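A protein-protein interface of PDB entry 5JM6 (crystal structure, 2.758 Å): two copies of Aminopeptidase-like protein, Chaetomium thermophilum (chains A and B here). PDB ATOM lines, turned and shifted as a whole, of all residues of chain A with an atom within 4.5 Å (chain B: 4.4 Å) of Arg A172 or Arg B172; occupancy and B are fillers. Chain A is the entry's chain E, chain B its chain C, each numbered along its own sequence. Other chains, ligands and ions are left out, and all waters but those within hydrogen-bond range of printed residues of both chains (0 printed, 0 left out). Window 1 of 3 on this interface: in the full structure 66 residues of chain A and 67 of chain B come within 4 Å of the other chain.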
ATOM      1  N   THR A 168     -11.718  -5.535  32.768  1.00  0.00           N
ATOM      2  CA  THR A 168     -11.808  -5.048  31.393  1.00  0.00           C
ATOM      3  C   THR A 168     -13.080  -4.247  31.111  1.00  0.00           C
ATOM      4  O   THR A 168     -13.205  -3.639  30.048  1.00  0.00           O
ATOM      5  CB  THR A 168     -11.728  -6.209  30.374  1.00  0.00           C
ATOM      6  OG1 THR A 168     -12.902  -7.025  30.469  1.00  0.00           O
ATOM      7  CG2 THR A 168     -10.493  -7.061  30.623  1.00  0.00           C
ATOM      8  N   TRP A 169     -14.014  -4.235  32.057  1.00  0.00           N
ATOM      9  CA  TRP A 169     -15.289  -3.550  31.854  1.00  0.00           C
ATOM     10  C   TRP A 169     -15.237  -2.054  32.176  1.00  0.00           C
ATOM     11  O   TRP A 169     -16.160  -1.315  31.837  1.00  0.00           O
ATOM     12  CB  TRP A 169     -16.386  -4.223  32.686  1.00  0.00           C
ATOM     13  CG  TRP A 169     -16.980  -5.424  32.010  1.00  0.00           C
ATOM     14  CD1 TRP A 169     -16.400  -6.651  31.860  1.00  0.00           C
ATOM     15  CD2 TRP A 169     -18.265  -5.508  31.382  1.00  0.00           C
ATOM     16  NE1 TRP A 169     -17.245  -7.493  31.179  1.00  0.00           N
ATOM     17  CE2 TRP A 169     -18.397  -6.817  30.874  1.00  0.00           C
ATOM     18  CE3 TRP A 169     -19.316  -4.605  31.199  1.00  0.00           C
ATOM     19  CZ2 TRP A 169     -19.538  -7.244  30.198  1.00  0.00           C
ATOM     20  CZ3 TRP A 169     -20.449  -5.031  30.528  1.00  0.00           C
ATOM     21  CH2 TRP A 169     -20.550  -6.339  30.036  1.00  0.00           C
ATOM     22  N   TRP A 170     -14.162  -1.606  32.820  1.00  0.00           N
ATOM     23  CA  TRP A 170     -14.027  -0.191  33.168  1.00  0.00           C
ATOM     24  C   TRP A 170     -13.785   0.676  31.932  1.00  0.00           C
ATOM     25  O   TRP A 170     -13.094   0.262  31.001  1.00  0.00           O
ATOM     26  CB  TRP A 170     -12.882   0.023  34.164  1.00  0.00           C
ATOM     27  CG  TRP A 170     -13.064  -0.604  35.521  1.00  0.00           C
ATOM     28  CD1 TRP A 170     -12.773  -1.889  35.869  1.00  0.00           C
ATOM     29  CD2 TRP A 170     -13.542   0.034  36.717  1.00  0.00           C
ATOM     30  NE1 TRP A 170     -13.049  -2.097  37.198  1.00  0.00           N
ATOM     31  CE2 TRP A 170     -13.523  -0.933  37.742  1.00  0.00           C
ATOM     32  CE3 TRP A 170     -13.990   1.326  37.018  1.00  0.00           C
ATOM     33  CZ2 TRP A 170     -13.934  -0.652  39.045  1.00  0.00           C
ATOM     34  CZ3 TRP A 170     -14.400   1.602  38.316  1.00  0.00           C
ATOM     35  CH2 TRP A 170     -14.368   0.616  39.311  1.00  0.00           C
ATOM     36  N   ASP A 171     -14.350   1.882  31.947  1.00  0.00           N
ATOM     37  CA  ASP A 171     -14.169   2.872  30.884  1.00  0.00           C
ATOM     38  C   ASP A 171     -14.387   2.307  29.481  1.00  0.00           C
ATOM     39  O   ASP A 171     -13.565   2.510  28.588  1.00  0.00           O
ATOM     40  CB  ASP A 171     -12.774   3.501  30.966  1.00  0.00           C
ATOM     41  CG  ASP A 171     -12.526   4.215  32.284  1.00  0.00           C
ATOM     42  OD1 ASP A 171     -13.507   4.552  32.978  1.00  0.00           O
ATOM     43  OD2 ASP A 171     -11.346   4.459  32.612  1.00  0.00           O
ATOM     44  N   ARG A 172     -15.491   1.591  29.300  1.00  0.00           N
ATOM     45  CA  ARG A 172     -15.887   1.098  27.986  1.00  0.00           C
ATOM     46  C   ARG A 172     -17.188   1.775  27.576  1.00  0.00           C
ATOM     47  O   ARG A 172     -18.002   2.121  28.434  1.00  0.00           O
ATOM     48  CB  ARG A 172     -16.060  -0.422  28.004  1.00  0.00           C
ATOM     49  CG  ARG A 172     -14.822  -1.189  28.437  1.00  0.00           C
ATOM     50  CD  ARG A 172     -13.905  -1.477  27.258  1.00  0.00           C
ATOM     51  NE  ARG A 172     -12.714  -2.214  27.671  1.00  0.00           N
ATOM     52  CZ  ARG A 172     -11.765  -2.634  26.839  1.00  0.00           C
ATOM     53  NH1 ARG A 172     -11.864  -2.397  25.537  1.00  0.00           N
ATOM     54  NH2 ARG A 172     -10.718  -3.296  27.312  1.00  0.00           N
ATOM     55  N   ASP A 173     -17.392   1.978  26.278  1.00  0.00           N
ATOM     56  CA  ASP A 173     -18.654   2.551  25.834  1.00  0.00           C
ATOM     57  C   ASP A 173     -19.688   1.440  25.849  1.00  0.00           C
ATOM     58  O   ASP A 173     -19.589   0.482  25.083  1.00  0.00           O
ATOM     59  CB  ASP A 173     -18.536   3.154  24.430  1.00  0.00           C
ATOM     60  CG  ASP A 173     -17.596   4.343  24.373  1.00  0.00           C
ATOM     61  OD1 ASP A 173     -16.932   4.639  25.387  1.00  0.00           O
ATOM     62  OD2 ASP A 173     -17.511   4.976  23.300  1.00  0.00           O
ATOM     63  N   LEU A 174     -20.695   1.578  26.702  1.00  0.00           N
ATOM     64  CA  LEU A 174     -21.682   0.522  26.861  1.00  0.00           C
ATOM     65  C   LEU A 174     -23.028   0.938  26.303  1.00  0.00           C
ATOM     66  O   LEU A 174     -23.493   2.056  26.530  1.00  0.00           O
ATOM     67  CB  LEU A 174     -21.834   0.125  28.331  1.00  0.00           C
ATOM     68  CG  LEU A 174     -20.579  -0.317  29.079  1.00  0.00           C
ATOM     69  CD1 LEU A 174     -20.917  -0.575  30.537  1.00  0.00           C
ATOM     70  CD2 LEU A 174     -19.966  -1.551  28.437  1.00  0.00           C
ATOM     71  N   ALA A 202     -24.224   4.057  28.529  1.00  0.00           N
ATOM     72  CA  ALA A 202     -23.756   3.744  29.874  1.00  0.00           C
ATOM     73  C   ALA A 202     -22.247   3.620  29.922  1.00  0.00           C
ATOM     74  O   ALA A 202     -21.599   3.353  28.910  1.00  0.00           O
ATOM     75  CB  ALA A 202     -24.405   2.461  30.378  1.00  0.00           C
ATOM     76  N   ARG A 203     -21.694   3.863  31.103  1.00  0.00           N
ATOM     77  CA  ARG A 203     -20.263   3.757  31.314  1.00  0.00           C
ATOM     78  C   ARG A 203     -19.932   3.498  32.780  1.00  0.00           C
ATOM     79  O   ARG A 203     -20.578   4.051  33.671  1.00  0.00           O
ATOM     80  CB  ARG A 203     -19.595   5.037  30.823  1.00  0.00           C
ATOM     81  CG  ARG A 203     -18.223   5.301  31.376  1.00  0.00           C
ATOM     82  CD  ARG A 203     -17.588   6.438  30.622  1.00  0.00           C
ATOM     83  NE  ARG A 203     -16.701   5.978  29.565  1.00  0.00           N
ATOM     84  CZ  ARG A 203     -15.379   6.086  29.617  1.00  0.00           C
ATOM     85  NH1 ARG A 203     -14.799   6.639  30.673  1.00  0.00           N
ATOM     86  NH2 ARG A 203     -14.641   5.640  28.611  1.00  0.00           N
ATOM     87  N   ILE A 487     -14.188  -8.317  28.072  1.00  0.00           N
ATOM     88  CA  ILE A 487     -15.280  -7.625  27.397  1.00  0.00           C
ATOM     89  C   ILE A 487     -14.956  -7.470  25.912  1.00  0.00           C
ATOM     90  O   ILE A 487     -15.846  -7.239  25.094  1.00  0.00           O
ATOM     91  CB  ILE A 487     -15.560  -6.239  28.017  1.00  0.00           C
ATOM     92  CG1 ILE A 487     -16.959  -5.754  27.629  1.00  0.00           C
ATOM     93  CG2 ILE A 487     -14.504  -5.232  27.594  1.00  0.00           C
ATOM     94  CD1 ILE A 487     -17.326  -4.409  28.212  1.00  0.00           C
ATOM     95  N   ARG A 488     -13.671  -7.550  25.578  1.00  0.00           N
ATOM     96  CA  ARG A 488     -13.235  -7.557  24.189  1.00  0.00           C
ATOM     97  C   ARG A 488     -12.079  -8.541  24.003  1.00  0.00           C
ATOM     98  O   ARG A 488     -10.997  -8.338  24.554  1.00  0.00           O
ATOM     99  CB  ARG A 488     -12.836  -6.143  23.768  1.00  0.00           C
ATOM    100  CG  ARG A 488     -12.628  -5.957  22.284  1.00  0.00           C
ATOM    101  CD  ARG A 488     -12.553  -4.484  21.929  1.00  0.00           C
ATOM    102  NE  ARG A 488     -12.344  -4.295  20.498  1.00  0.00           N
ATOM    103  CZ  ARG A 488     -13.320  -4.110  19.615  1.00  0.00           C
ATOM    104  NH1 ARG A 488     -14.584  -4.080  20.015  1.00  0.00           N
ATOM    105  NH2 ARG A 488     -13.030  -3.952  18.332  1.00  0.00           N
ATOM    106  N   THR B 168      -6.194   0.122  32.289  1.00  0.00           N
ATOM    107  CA  THR B 168      -7.174   0.453  31.255  1.00  0.00           C
ATOM    108  C   THR B 168      -6.638   0.206  29.843  1.00  0.00           C
ATOM    109  O   THR B 168      -7.395   0.266  28.876  1.00  0.00           O
ATOM    110  CB  THR B 168      -7.661   1.922  31.350  1.00  0.00           C
ATOM    111  OG1 THR B 168      -6.593   2.821  31.028  1.00  0.00           O
ATOM    112  CG2 THR B 168      -8.194   2.227  32.740  1.00  0.00           C
ATOM    113  N   TRP B 169      -5.347  -0.090  29.718  1.00  0.00           N
ATOM    114  CA  TRP B 169      -4.751  -0.291  28.398  1.00  0.00           C
ATOM    115  C   TRP B 169      -4.928  -1.711  27.847  1.00  0.00           C
ATOM    116  O   TRP B 169      -4.726  -1.939  26.655  1.00  0.00           O
ATOM    117  CB  TRP B 169      -3.262   0.073  28.431  1.00  0.00           C
ATOM    118  CG  TRP B 169      -3.022   1.548  28.290  1.00  0.00           C
ATOM    119  CD1 TRP B 169      -3.260   2.508  29.227  1.00  0.00           C
ATOM    120  CD2 TRP B 169      -2.505   2.230  27.139  1.00  0.00           C
ATOM    121  NE1 TRP B 169      -2.925   3.746  28.733  1.00  0.00           N
ATOM    122  CE2 TRP B 169      -2.458   3.602  27.453  1.00  0.00           C
ATOM    123  CE3 TRP B 169      -2.079   1.814  25.874  1.00  0.00           C
ATOM    124  CZ2 TRP B 169      -2.002   4.561  26.551  1.00  0.00           C
ATOM    125  CZ3 TRP B 169      -1.626   2.768  24.978  1.00  0.00           C
ATOM    126  CH2 TRP B 169      -1.591   4.125  25.321  1.00  0.00           C
ATOM    127  N   TRP B 170      -5.315  -2.658  28.698  1.00  0.00           N
ATOM    128  CA  TRP B 170      -5.498  -4.039  28.251  1.00  0.00           C
ATOM    129  C   TRP B 170      -6.707  -4.191  27.330  1.00  0.00           C
ATOM    130  O   TRP B 170      -7.753  -3.585  27.563  1.00  0.00           O
ATOM    131  CB  TRP B 170      -5.665  -4.980  29.441  1.00  0.00           C
ATOM    132  CG  TRP B 170      -4.481  -5.097  30.347  1.00  0.00           C
ATOM    133  CD1 TRP B 170      -4.158  -4.264  31.376  1.00  0.00           C
ATOM    134  CD2 TRP B 170      -3.480  -6.126  30.336  1.00  0.00           C
ATOM    135  NE1 TRP B 170      -3.013  -4.698  31.997  1.00  0.00           N
ATOM    136  CE2 TRP B 170      -2.577  -5.839  31.377  1.00  0.00           C
ATOM    137  CE3 TRP B 170      -3.256  -7.255  29.541  1.00  0.00           C
ATOM    138  CZ2 TRP B 170      -1.469  -6.640  31.647  1.00  0.00           C
ATOM    139  CZ3 TRP B 170      -2.153  -8.049  29.811  1.00  0.00           C
ATOM    140  CH2 TRP B 170      -1.273  -7.736  30.854  1.00  0.00           C
ATOM    141  N   ASP B 171      -6.555  -5.022  26.301  1.00  0.00           N
ATOM    142  CA  ASP B 171      -7.626  -5.321  25.350  1.00  0.00           C
ATOM    143  C   ASP B 171      -8.247  -4.064  24.750  1.00  0.00           C
ATOM    144  O   ASP B 171      -9.468  -3.904  24.737  1.00  0.00           O
ATOM    145  CB  ASP B 171      -8.713  -6.171  26.013  1.00  0.00           C
ATOM    146  CG  ASP B 171      -8.207  -7.531  26.442  1.00  0.00           C
ATOM    147  OD1 ASP B 171      -7.289  -8.065  25.784  1.00  0.00           O
ATOM    148  OD2 ASP B 171      -8.738  -8.072  27.434  1.00  0.00           O
ATOM    149  N   ARG B 172      -7.392  -3.170  24.268  1.00  0.00           N
ATOM    150  CA  ARG B 172      -7.830  -2.001  23.520  1.00  0.00           C
ATOM    151  C   ARG B 172      -7.315  -2.116  22.092  1.00  0.00           C
ATOM    152  O   ARG B 172      -6.239  -2.670  21.865  1.00  0.00           O
ATOM    153  CB  ARG B 172      -7.322  -0.712  24.171  1.00  0.00           C
ATOM    154  CG  ARG B 172      -7.745  -0.531  25.619  1.00  0.00           C
ATOM    155  CD  ARG B 172      -9.143   0.059  25.722  1.00  0.00           C
ATOM    156  NE  ARG B 172      -9.549   0.239  27.114  1.00  0.00           N
ATOM    157  CZ  ARG B 172     -10.720   0.737  27.495  1.00  0.00           C
ATOM    158  NH1 ARG B 172     -11.611   1.114  26.588  1.00  0.00           N
ATOM    159  NH2 ARG B 172     -10.998   0.860  28.786  1.00  0.00           N
ATOM    160  N   ASP B 173      -8.061  -1.582  21.130  1.00  0.00           N
ATOM    161  CA  ASP B 173      -7.591  -1.628  19.755  1.00  0.00           C
ATOM    162  C   ASP B 173      -6.621  -0.468  19.592  1.00  0.00           C
ATOM    163  O   ASP B 173      -7.021   0.695  19.629  1.00  0.00           O
ATOM    164  CB  ASP B 173      -8.749  -1.509  18.754  1.00  0.00           C
ATOM    165  CG  ASP B 173      -9.751  -2.655  18.856  1.00  0.00           C
ATOM    166  OD1 ASP B 173      -9.721  -3.404  19.854  1.00  0.00           O
ATOM    167  OD2 ASP B 173     -10.581  -2.798  17.931  1.00  0.00           O
ATOM    168  N   LEU B 174      -5.349  -0.786  19.384  1.00  0.00           N
ATOM    169  CA  LEU B 174      -4.319   0.242  19.353  1.00  0.00           C
ATOM    170  C   LEU B 174      -3.862   0.507  17.933  1.00  0.00           C
ATOM    171  O   LEU B 174      -3.679  -0.418  17.142  1.00  0.00           O
ATOM    172  CB  LEU B 174      -3.122  -0.153  20.224  1.00  0.00           C
ATOM    173  CG  LEU B 174      -3.423  -0.405  21.702  1.00  0.00           C
ATOM    174  CD1 LEU B 174      -2.200  -0.948  22.435  1.00  0.00           C
ATOM    175  CD2 LEU B 174      -3.928   0.870  22.361  1.00  0.00           C
ATOM    176  N   ALA B 202      -2.215  -2.940  16.783  1.00  0.00           N
ATOM    177  CA  ALA B 202      -1.557  -3.402  17.997  1.00  0.00           C
ATOM    178  C   ALA B 202      -2.560  -3.678  19.094  1.00  0.00           C
ATOM    179  O   ALA B 202      -3.653  -3.111  19.112  1.00  0.00           O
ATOM    180  CB  ALA B 202      -0.531  -2.381  18.468  1.00  0.00           C
ATOM    181  N   ARG B 203      -2.200  -4.592  19.981  1.00  0.00           N
ATOM    182  CA  ARG B 203      -3.065  -4.934  21.090  1.00  0.00           C
ATOM    183  C   ARG B 203      -2.274  -5.540  22.245  1.00  0.00           C
ATOM    184  O   ARG B 203      -1.298  -6.256  22.020  1.00  0.00           O
ATOM    185  CB  ARG B 203      -4.146  -5.890  20.595  1.00  0.00           C
ATOM    186  CG  ARG B 203      -5.027  -6.449  21.664  1.00  0.00           C
ATOM    187  CD  ARG B 203      -6.404  -6.684  21.118  1.00  0.00           C
ATOM    188  NE  ARG B 203      -7.209  -7.469  22.038  1.00  0.00           N
ATOM    189  CZ  ARG B 203      -8.487  -7.226  22.287  1.00  0.00           C
ATOM    190  NH1 ARG B 203      -9.097  -6.215  21.683  1.00  0.00           N
ATOM    191  NH2 ARG B 203      -9.152  -7.989  23.141  1.00  0.00           N
ATOM    192  N   ILE B 487      -6.902   5.386  29.437  1.00  0.00           N
ATOM    193  CA  ILE B 487      -6.735   5.395  27.990  1.00  0.00           C
ATOM    194  C   ILE B 487      -8.002   5.934  27.329  1.00  0.00           C
ATOM    195  O   ILE B 487      -7.979   6.346  26.170  1.00  0.00           O
ATOM    196  CB  ILE B 487      -6.407   3.992  27.428  1.00  0.00           C
ATOM    197  CG1 ILE B 487      -5.783   4.112  26.034  1.00  0.00           C
ATOM    198  CG2 ILE B 487      -7.648   3.111  27.394  1.00  0.00           C
ATOM    199  CD1 ILE B 487      -5.436   2.789  25.394  1.00  0.00           C
ATOM    200  N   ARG B 488      -9.119   5.877  28.050  1.00  0.00           N
ATOM    201  CA  ARG B 488     -10.353   6.505  27.596  1.00  0.00           C
ATOM    202  C   ARG B 488     -11.110   7.151  28.760  1.00  0.00           C
ATOM    203  O   ARG B 488     -11.603   6.450  29.642  1.00  0.00           O
ATOM    204  CB  ARG B 488     -11.221   5.467  26.891  1.00  0.00           C
ATOM    205  CG  ARG B 488     -12.406   6.033  26.147  1.00  0.00           C
ATOM    206  CD  ARG B 488     -13.002   4.978  25.237  1.00  0.00           C
ATOM    207  NE  ARG B 488     -14.129   5.492  24.468  1.00  0.00           N
ATOM    208  CZ  ARG B 488     -14.026   6.023  23.255  1.00  0.00           C
ATOM    209  NH1 ARG B 488     -12.842   6.116  22.665  1.00  0.00           N
ATOM    210  NH2 ARG B 488     -15.109   6.464  22.630  1.00  0.00           N
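Arg A172 touches three residues of chain B. Printed residues of chain B within 4 Å of Asp A173: Arg B488. Arg B172 touches just these residues of chain A: Trp A170, Asp A171 and Arg A172. Of the printed residues of chain A, Arg B203 touches Arg A488. The nearest printed residue of chain A that does not touch Arg B172 is Thr A168 (5.2 Å).
Of the 11 printed residues of chain A, 7 touch a printed residue of chain B. Of the 11 printed residues of chain B, 7 touch a printed residue of chain A. Printed residues of chain B that touch a printed residue of chain A: Thr B168, Trp B170, Asp B171, Arg B172, Asp B173, Arg B203 and Arg B488. Among the printed residues, Asp or Glu carboxylates within 4 Å of a Lys or Arg side-chain nitrogen of the other chain: Asp A173 with Arg B488 (2.9 Å) and Arg A488 with Asp B173 (2.7 Å).
CG2 of Thr A168 touches OD2 of Asp B171, 3.8 Å away. Asp A171 touches Thr B168 (OD2 to CG2, 3.9 Å). CB of Asp A171 touches O of Arg B488, at 3.4 Å. Arg A172 touches Arg B172. Arg A488 touches Asp B171 (O to CG, 3.5 Å).
The guanidinium group of Arg A203 lies within hydrogen-bond range of the backbone carbonyl oxygen of Arg B488 (3.3 Å). The side-chain carboxylate of Asp A173 is in salt-bridge range of the guanidinium group of Arg B488, at 2.9 Å. The backbone carbonyl oxygen (O) of Trp A170 is in hydrogen-bond range of the guanidinium group (NH2) of Arg B172 (3.1 Å). O of Asp A171 is in hydrogen-bond range of NH2 of Arg B172, 3.1 Å away. The backbone carbonyl oxygen of Arg A488 lies close to the guanidinium group of Arg B203, 2.3 Å away. The backbone carbonyl oxygen (O) of Asp B171 lies within hydrogen-bond range of the guanidinium group (NH2) of Arg A172 (2.9 Å). The backbone carbonyl oxygen (O) of Trp B170 is in hydrogen-bond range of the guanidinium group (NH2) of Arg A172, 3.0 Å away. The guanidinium group (NH2) of Arg A488 is in salt-bridge range of the side-chain carboxylate (OD2) of Asp B173, at 2.7 Å.
OG1 of Thr A168 lies within hydrogen-bond range of N of Ile A487 (3.0 Å). OD1 of Asp B173 lies within salt-bridge range of NH1 of Arg B203, 3.4 Å away. O of Thr A168 is in hydrogen-bond range of NE of Arg A172 (2.8 Å). OG1 of Thr B168 lies within hydrogen-bond range of N of Ile B487 (3.0 Å). The guanidinium group of Arg B203 lies within salt-bridge range of the side-chain carboxylate of Asp B171 (3.2 Å). O of Thr B168 sits at hydrogen-bond distance from NE of Arg B172 (2.8 Å).
Thr A168 touches Asp B171, and with the chains exchanged Asp A171 touches Thr B168. Trp A170 touches Arg B172, and with the chains exchanged Arg A172 touches Trp B170. Asp A171 touches Arg B488, and with the chains exchanged Arg A488 touches Asp B171. Arg A203 touches Arg B488, and with the chains exchanged Arg A488 touches Arg B203. Of the 13 pairs that touch across the chains among the printed residues, 13 have their exchanged pair printed and touching as well.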
